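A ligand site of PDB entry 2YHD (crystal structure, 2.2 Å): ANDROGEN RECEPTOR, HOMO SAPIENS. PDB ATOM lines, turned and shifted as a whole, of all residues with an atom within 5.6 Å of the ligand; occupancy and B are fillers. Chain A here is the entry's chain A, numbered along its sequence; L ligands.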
ATOM      1  N   LEU A  31      31.311 -25.565  14.520  1.00  0.00           N
ATOM      2  CA  LEU A  31      30.215 -25.634  13.536  1.00  0.00           C
ATOM      3  C   LEU A  31      28.913 -26.160  14.173  1.00  0.00           C
ATOM      4  O   LEU A  31      27.829 -25.708  13.768  1.00  0.00           O
ATOM      5  CB  LEU A  31      30.586 -26.411  12.245  1.00  0.00           C
ATOM      6  CG  LEU A  31      31.218 -25.622  11.084  1.00  0.00           C
ATOM      7  CD1 LEU A  31      30.244 -24.631  10.462  1.00  0.00           C
ATOM      8  CD2 LEU A  31      32.465 -24.845  11.468  1.00  0.00           C
ATOM      9  N   LEU A  34      27.432 -23.138  15.824  1.00  0.00           N
ATOM     10  CA  LEU A  34      26.920 -22.221  14.769  1.00  0.00           C
ATOM     11  C   LEU A  34      25.570 -22.709  14.323  1.00  0.00           C
ATOM     12  O   LEU A  34      24.617 -21.919  14.222  1.00  0.00           O
ATOM     13  CB  LEU A  34      27.887 -22.095  13.541  1.00  0.00           C
ATOM     14  CG  LEU A  34      29.007 -21.054  13.596  1.00  0.00           C
ATOM     15  CD1 LEU A  34      29.783 -20.997  12.298  1.00  0.00           C
ATOM     16  CD2 LEU A  34      28.525 -19.667  13.898  1.00  0.00           C
ATOM     17  N   ASN A  35      25.490 -24.020  14.071  1.00  0.00           N
ATOM     18  CA  ASN A  35      24.235 -24.747  13.783  1.00  0.00           C
ATOM     19  C   ASN A  35      23.161 -24.609  14.895  1.00  0.00           C
ATOM     20  O   ASN A  35      21.967 -24.391  14.597  1.00  0.00           O
ATOM     21  CB  ASN A  35      24.516 -26.243  13.569  1.00  0.00           C
ATOM     22  CG  ASN A  35      25.167 -26.536  12.249  1.00  0.00           C
ATOM     23  OD1 ASN A  35      25.263 -25.672  11.357  1.00  0.00           O
ATOM     24  ND2 ASN A  35      25.635 -27.794  12.104  1.00  0.00           N
ATOM     25  N   LEU A  37      23.030 -22.148  17.111  1.00  0.00           N
ATOM     26  CA  LEU A  37      22.734 -20.759  17.015  1.00  0.00           C
ATOM     27  C   LEU A  37      21.786 -20.489  15.829  1.00  0.00           C
ATOM     28  O   LEU A  37      20.839 -19.701  15.977  1.00  0.00           O
ATOM     29  CB  LEU A  37      24.047 -19.978  16.797  1.00  0.00           C
ATOM     30  CG  LEU A  37      23.729 -18.488  16.642  1.00  0.00           C
ATOM     31  CD1 LEU A  37      23.164 -17.918  17.972  1.00  0.00           C
ATOM     32  CD2 LEU A  37      24.976 -17.776  16.219  1.00  0.00           C
ATOM     33  N   GLY A  38      22.032 -21.073  14.655  1.00  0.00           N
ATOM     34  CA  GLY A  38      21.118 -20.874  13.553  1.00  0.00           C
ATOM     35  C   GLY A  38      19.750 -21.347  13.966  1.00  0.00           C
ATOM     36  O   GLY A  38      18.754 -20.654  13.748  1.00  0.00           O
ATOM     37  N   GLN A  41      18.146 -18.733  16.397  1.00  0.00           N
ATOM     38  CA  GLN A  41      17.754 -17.571  15.612  1.00  0.00           C
ATOM     39  C   GLN A  41      16.543 -17.776  14.688  1.00  0.00           C
ATOM     40  O   GLN A  41      15.822 -16.831  14.498  1.00  0.00           O
ATOM     41  CB  GLN A  41      18.923 -16.958  14.864  1.00  0.00           C
ATOM     42  CG  GLN A  41      19.932 -16.331  15.791  1.00  0.00           C
ATOM     43  CD  GLN A  41      20.965 -15.523  15.030  1.00  0.00           C
ATOM     44  OE1 GLN A  41      20.786 -15.171  13.838  1.00  0.00           O
ATOM     45  NE2 GLN A  41      22.081 -15.249  15.688  1.00  0.00           N
ATOM     46  N   TRP A  71      16.402 -16.872   5.310  1.00  0.00           N
ATOM     47  CA  TRP A  71      16.992 -16.817   6.629  1.00  0.00           C
ATOM     48  C   TRP A  71      18.505 -16.573   6.612  1.00  0.00           C
ATOM     49  O   TRP A  71      19.010 -15.804   7.383  1.00  0.00           O
ATOM     50  CB  TRP A  71      16.641 -18.063   7.438  1.00  0.00           C
ATOM     51  CG  TRP A  71      17.080 -19.328   6.781  1.00  0.00           C
ATOM     52  CD1 TRP A  71      16.370 -20.046   5.857  1.00  0.00           C
ATOM     53  CD2 TRP A  71      18.310 -20.045   6.985  1.00  0.00           C
ATOM     54  NE1 TRP A  71      17.075 -21.155   5.467  1.00  0.00           N
ATOM     55  CE2 TRP A  71      18.262 -21.202   6.139  1.00  0.00           C
ATOM     56  CE3 TRP A  71      19.438 -19.849   7.814  1.00  0.00           C
ATOM     57  CZ2 TRP A  71      19.300 -22.154   6.079  1.00  0.00           C
ATOM     58  CZ3 TRP A  71      20.470 -20.782   7.764  1.00  0.00           C
ATOM     59  CH2 TRP A  71      20.394 -21.954   6.886  1.00  0.00           C
ATOM     60  N   MET A  72      19.222 -17.207   5.683  1.00  0.00           N
ATOM     61  CA  MET A  72      20.699 -17.087   5.625  1.00  0.00           C
ATOM     62  C   MET A  72      21.137 -15.646   5.403  1.00  0.00           C
ATOM     63  O   MET A  72      22.044 -15.171   6.070  1.00  0.00           O
ATOM     64  CB  MET A  72      21.377 -18.040   4.566  1.00  0.00           C
ATOM     65  CG  MET A  72      22.899 -17.817   4.514  1.00  0.00           C
ATOM     66  SD  MET A  72      23.531 -18.791   5.907  1.00  0.00           S
ATOM     67  CE  MET A  72      23.190 -20.462   5.363  1.00  0.00           C
ATOM     68  N   MET A  75      20.163 -13.345   8.615  1.00  0.00           N
ATOM     69  CA  MET A  75      21.113 -13.546   9.698  1.00  0.00           C
ATOM     70  C   MET A  75      22.529 -13.089   9.391  1.00  0.00           C
ATOM     71  O   MET A  75      23.147 -12.536  10.260  1.00  0.00           O
ATOM     72  CB  MET A  75      21.146 -14.992  10.135  1.00  0.00           C
ATOM     73  CG  MET A  75      19.781 -15.482  10.616  1.00  0.00           C
ATOM     74  SD  MET A  75      19.792 -17.250  10.933  1.00  0.00           S
ATOM     75  CE  MET A  75      18.080 -17.490  11.351  1.00  0.00           C
ATOM     76  N   VAL A  76      23.022 -13.277   8.151  1.00  0.00           N
ATOM     77  CA  VAL A  76      24.359 -12.734   7.779  1.00  0.00           C
ATOM     78  C   VAL A  76      24.348 -11.211   7.895  1.00  0.00           C
ATOM     79  O   VAL A  76      25.282 -10.567   8.442  1.00  0.00           O
ATOM     80  CB  VAL A  76      24.736 -13.173   6.356  1.00  0.00           C
ATOM     81  CG1 VAL A  76      25.939 -12.395   5.808  1.00  0.00           C
ATOM     82  CG2 VAL A  76      25.078 -14.638   6.385  1.00  0.00           C
ATOM     83  N   MET A  79      24.127 -10.148  11.635  1.00  0.00           N
ATOM     84  CA  MET A  79      25.423 -10.456  12.258  1.00  0.00           C
ATOM     85  C   MET A  79      26.512  -9.395  11.902  1.00  0.00           C
ATOM     86  O   MET A  79      27.390  -9.092  12.730  1.00  0.00           O
ATOM     87  CB  MET A  79      25.901 -11.824  11.818  1.00  0.00           C
ATOM     88  CG  MET A  79      27.091 -12.329  12.605  1.00  0.00           C
ATOM     89  SD  MET A  79      28.669 -11.794  11.913  1.00  0.00           S
ATOM     90  CE  MET A  79      28.871 -13.013  10.615  1.00  0.00           C
ATOM     91  N   ARG A  82      25.763  -6.446  13.962  1.00  0.00           N
ATOM     92  CA  ARG A  82      26.267  -6.639  15.330  1.00  0.00           C
ATOM     93  C   ARG A  82      27.789  -6.525  15.424  1.00  0.00           C
ATOM     94  O   ARG A  82      28.310  -5.951  16.372  1.00  0.00           O
ATOM     95  CB  ARG A  82      25.877  -8.001  15.862  1.00  0.00           C
ATOM     96  CG  ARG A  82      24.415  -8.077  16.275  1.00  0.00           C
ATOM     97  CD  ARG A  82      24.140  -9.422  17.021  1.00  0.00           C
ATOM     98  NE  ARG A  82      24.683 -10.554  16.285  1.00  0.00           N
ATOM     99  CZ  ARG A  82      23.972 -11.315  15.446  1.00  0.00           C
ATOM    100  NH1 ARG A  82      22.669 -11.084  15.227  1.00  0.00           N
ATOM    101  NH2 ARG A  82      24.575 -12.291  14.795  1.00  0.00           N
ATOM    102  N   PHE A  94      28.900 -13.409  16.006  1.00  0.00           N
ATOM    103  CA  PHE A  94      27.809 -14.321  15.875  1.00  0.00           C
ATOM    104  C   PHE A  94      26.876 -14.196  17.062  1.00  0.00           C
ATOM    105  O   PHE A  94      25.662 -14.045  16.856  1.00  0.00           O
ATOM    106  CB  PHE A  94      28.329 -15.755  15.709  1.00  0.00           C
ATOM    107  CG  PHE A  94      28.944 -15.975  14.385  1.00  0.00           C
ATOM    108  CD1 PHE A  94      28.142 -16.113  13.250  1.00  0.00           C
ATOM    109  CD2 PHE A  94      30.304 -16.030  14.253  1.00  0.00           C
ATOM    110  CE1 PHE A  94      28.724 -16.300  11.965  1.00  0.00           C
ATOM    111  CE2 PHE A  94      30.920 -16.221  12.990  1.00  0.00           C
ATOM    112  CZ  PHE A  94      30.104 -16.344  11.823  1.00  0.00           C
ATOM    113  N   MET A 110      36.042 -21.952   7.262  1.00  0.00           N
ATOM    114  CA  MET A 110      35.275 -21.075   6.391  1.00  0.00           C
ATOM    115  C   MET A 110      35.989 -19.782   6.307  1.00  0.00           C
ATOM    116  O   MET A 110      35.342 -18.706   6.306  1.00  0.00           O
ATOM    117  CB  MET A 110      33.902 -20.748   6.982  1.00  0.00           C
ATOM    118  CG  MET A 110      33.089 -21.869   7.510  1.00  0.00           C
ATOM    119  SD  MET A 110      31.504 -21.111   7.917  1.00  0.00           S
ATOM    120  CE  MET A 110      31.725 -20.626   9.627  1.00  0.00           C
ATOM    121  N   MET A 117      32.289 -11.885   4.938  1.00  0.00           N
ATOM    122  CA  MET A 117      31.422 -11.370   6.004  1.00  0.00           C
ATOM    123  C   MET A 117      32.051 -10.193   6.768  1.00  0.00           C
ATOM    124  O   MET A 117      31.330  -9.201   7.125  1.00  0.00           O
ATOM    125  CB  MET A 117      31.044 -12.491   6.950  1.00  0.00           C
ATOM    126  CG  MET A 117      30.047 -13.527   6.298  1.00  0.00           C
ATOM    127  SD  MET A 117      29.377 -14.787   7.412  1.00  0.00           S
ATOM    128  CE  MET A 117      30.696 -16.037   7.453  1.00  0.00           C
ATOM    129  N   LEU A 203      27.450 -19.571   1.614  1.00  0.00           N
ATOM    130  CA  LEU A 203      27.198 -20.317   2.862  1.00  0.00           C
ATOM    131  C   LEU A 203      26.132 -21.389   2.643  1.00  0.00           C
ATOM    132  O   LEU A 203      26.099 -22.398   3.338  1.00  0.00           O
ATOM    133  CB  LEU A 203      26.830 -19.386   4.030  1.00  0.00           C
ATOM    134  CG  LEU A 203      27.892 -18.299   4.276  1.00  0.00           C
ATOM    135  CD1 LEU A 203      27.284 -17.077   4.815  1.00  0.00           C
ATOM    136  CD2 LEU A 203      29.047 -18.782   5.176  1.00  0.00           C
ATOM    137  N   PHE A 206      28.280 -24.342   1.289  1.00  0.00           N
ATOM    138  CA  PHE A 206      29.004 -24.843   2.461  1.00  0.00           C
ATOM    139  C   PHE A 206      28.193 -25.733   3.474  1.00  0.00           C
ATOM    140  O   PHE A 206      28.521 -26.933   3.722  1.00  0.00           O
ATOM    141  CB  PHE A 206      29.803 -23.665   3.131  1.00  0.00           C
ATOM    142  CG  PHE A 206      30.736 -24.121   4.212  1.00  0.00           C
ATOM    143  CD1 PHE A 206      30.218 -24.568   5.447  1.00  0.00           C
ATOM    144  CD2 PHE A 206      32.114 -24.149   4.003  1.00  0.00           C
ATOM    145  CE1 PHE A 206      31.059 -25.026   6.466  1.00  0.00           C
ATOM    146  CE2 PHE A 206      32.971 -24.592   5.018  1.00  0.00           C
ATOM    147  CZ  PHE A 206      32.444 -25.028   6.268  1.00  0.00           C
ATOM    148  N   THR A 207      27.132 -25.175   4.033  1.00  0.00           N
ATOM    149  CA  THR A 207      26.316 -25.900   4.991  1.00  0.00           C
ATOM    150  C   THR A 207      25.606 -27.120   4.361  1.00  0.00           C
ATOM    151  O   THR A 207      25.377 -28.161   5.037  1.00  0.00           O
ATOM    152  CB  THR A 207      25.262 -24.963   5.703  1.00  0.00           C
ATOM    153  OG1 THR A 207      24.732 -25.678   6.813  1.00  0.00           O
ATOM    154  CG2 THR A 207      24.014 -24.593   4.778  1.00  0.00           C
ATOM    155  N   LEU A 210      28.252 -29.711   4.136  1.00  0.00           N
ATOM    156  CA  LEU A 210      28.544 -30.200   5.517  1.00  0.00           C
ATOM    157  C   LEU A 210      27.456 -31.139   6.004  1.00  0.00           C
ATOM    158  O   LEU A 210      27.772 -32.151   6.584  1.00  0.00           O
ATOM    159  CB  LEU A 210      28.728 -29.013   6.472  1.00  0.00           C
ATOM    160  CG  LEU A 210      28.981 -29.122   7.965  1.00  0.00           C
ATOM    161  CD1 LEU A 210      30.178 -30.069   8.233  1.00  0.00           C
ATOM    162  CD2 LEU A 210      29.353 -27.752   8.405  1.00  0.00           C
ATOM    163  N   PHE A 221      23.548 -31.155  13.516  1.00  0.00           N
ATOM    164  CA  PHE A 221      22.530 -30.242  12.965  1.00  0.00           C
ATOM    165  C   PHE A 221      21.271 -30.567  13.739  1.00  0.00           C
ATOM    166  O   PHE A 221      20.861 -31.737  13.783  1.00  0.00           O
ATOM    167  CB  PHE A 221      22.291 -30.555  11.500  1.00  0.00           C
ATOM    168  CG  PHE A 221      23.364 -30.068  10.600  1.00  0.00           C
ATOM    169  CD1 PHE A 221      24.540 -30.803  10.421  1.00  0.00           C
ATOM    170  CD2 PHE A 221      23.241 -28.851   9.926  1.00  0.00           C
ATOM    171  CE1 PHE A 221      25.565 -30.326   9.556  1.00  0.00           C
ATOM    172  CE2 PHE A 221      24.271 -28.384   9.071  1.00  0.00           C
ATOM    173  CZ  PHE A 221      25.386 -29.124   8.875  1.00  0.00           C
ATOM    174  N   MET A 225      17.230 -27.118  11.267  1.00  0.00           N
ATOM    175  CA  MET A 225      18.314 -26.796  10.356  1.00  0.00           C
ATOM    176  C   MET A 225      18.447 -27.950   9.380  1.00  0.00           C
ATOM    177  O   MET A 225      18.478 -27.737   8.188  1.00  0.00           O
ATOM    178  CB  MET A 225      19.649 -26.527  11.100  1.00  0.00           C
ATOM    179  CG  MET A 225      19.648 -25.268  11.967  1.00  0.00           C
ATOM    180  SD  MET A 225      19.637 -23.792  10.966  1.00  0.00           S
ATOM    181  CE  MET A 225      21.414 -23.633  10.710  1.00  0.00           C
ATOM    182  N   ILE A 229      17.776 -27.516   5.430  1.00  0.00           N
ATOM    183  CA  ILE A 229      19.021 -27.647   4.611  1.00  0.00           C
ATOM    184  C   ILE A 229      18.931 -28.781   3.577  1.00  0.00           C
ATOM    185  O   ILE A 229      19.573 -28.717   2.523  1.00  0.00           O
ATOM    186  CB  ILE A 229      20.298 -27.661   5.485  1.00  0.00           C
ATOM    187  CG1 ILE A 229      20.420 -26.305   6.216  1.00  0.00           C
ATOM    188  CG2 ILE A 229      21.567 -27.905   4.626  1.00  0.00           C
ATOM    189  CD1 ILE A 229      21.547 -26.266   7.239  1.00  0.00           C
HETATM  190  C1  LIG L   1      24.078 -18.469  12.371  1.00  0.00           C
HETATM  191  C2  LIG L   1      23.460 -17.148  12.834  1.00  0.00           C
HETATM  192  C3  LIG L   1      24.396 -16.058  12.425  1.00  0.00           C
HETATM  193  O1  LIG L   1      24.520 -15.039  13.127  1.00  0.00           O
HETATM  194  C4  LIG L   1      25.158 -16.243  11.158  1.00  0.00           C
HETATM  195  C5  LIG L   1      25.198 -17.391  10.436  1.00  0.00           C
HETATM  196  C6  LIG L   1      26.161 -17.453   9.234  1.00  0.00           C
HETATM  197  C7  LIG L   1      26.805 -18.843   8.997  1.00  0.00           C
HETATM  198  C8  LIG L   1      25.868 -20.005   9.228  1.00  0.00           C
HETATM  199  C9  LIG L   1      25.135 -19.885  10.585  1.00  0.00           C
HETATM  200  C10 LIG L   1      24.344 -18.574  10.850  1.00  0.00           C
HETATM  201  C11 LIG L   1      24.286 -21.120  10.944  1.00  0.00           C
HETATM  202  C12 LIG L   1      24.981 -22.481  10.689  1.00  0.00           C
HETATM  203  C13 LIG L   1      25.730 -22.495   9.345  1.00  0.00           C
HETATM  204  C14 LIG L   1      26.657 -21.317   9.261  1.00  0.00           C
HETATM  205  C15 LIG L   1      27.651 -21.671   8.123  1.00  0.00           C
HETATM  206  C16 LIG L   1      27.750 -23.198   8.127  1.00  0.00           C
HETATM  207  C17 LIG L   1      26.780 -23.590   9.219  1.00  0.00           C
HETATM  208  O2  LIG L   1      26.200 -24.857   9.008  1.00  0.00           O
HETATM  209  C18 LIG L   1      24.693 -22.414   8.206  1.00  0.00           C
HETATM  210  C19 LIG L   1      22.971 -18.596  10.137  1.00  0.00           C
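The side-chain amide nitrogen (ND2) of Asn 35 sits close to the backbone carbonyl oxygen (O) of Leu 31 (3.5 Å).
The backbone carbonyl oxygen (O) of Phe 94 sits at hydrogen-bond distance from the guanidinium group (NH2) of Arg 82 (2.9 Å).
SD of Met 75 lies close to OE1 of Gln 41.
CD1 of Leu 31 touches C16 of the ligand, at 3.7 Å.
Leu 34 touches the ligand (O to C11, 3.4 Å).
Leu 37 touches the ligand (CD2 to C2, 3.8 Å).
Gly 38 touches the ligand (CA to C1, 3.99 Å).
OE1 of Gln 41 touches C2 of the ligand, 3.5 Å away.
CE of Met 72 touches C18 of the ligand (3.8 Å).
Met 75 touches the ligand.
CB of Met 79 touches O1 of the ligand, 3.7 Å away.
Phe 94 touches the ligand.
SD of Met 110 touches C15 of the ligand (3.9 Å).
Phe 206 touches the ligand.
Met 225 touches the ligand.
Hydrophobic or aromatic side chains within 4 Å of the ligand: Leu 31, Leu 37, Met 72, Met 75, Met 79, Phe 94, Met 110, Phe 206 and Met 225.
The nearest printed residue that does not touch the ligand is Phe 221 (4.02 Å).
OD1 of Asn 35 lies within hydrogen-bond range of O2 of the ligand, at 2.7 Å.
The side-chain hydroxyl of Thr 207 lies within hydrogen-bond range of an oxygen (O2) of the ligand, at 2.8 Å.
An oxygen (O1) of the ligand is in hydrogen-bond range of the guanidinium group (NH2) of Arg 82, at 3.2 Å.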
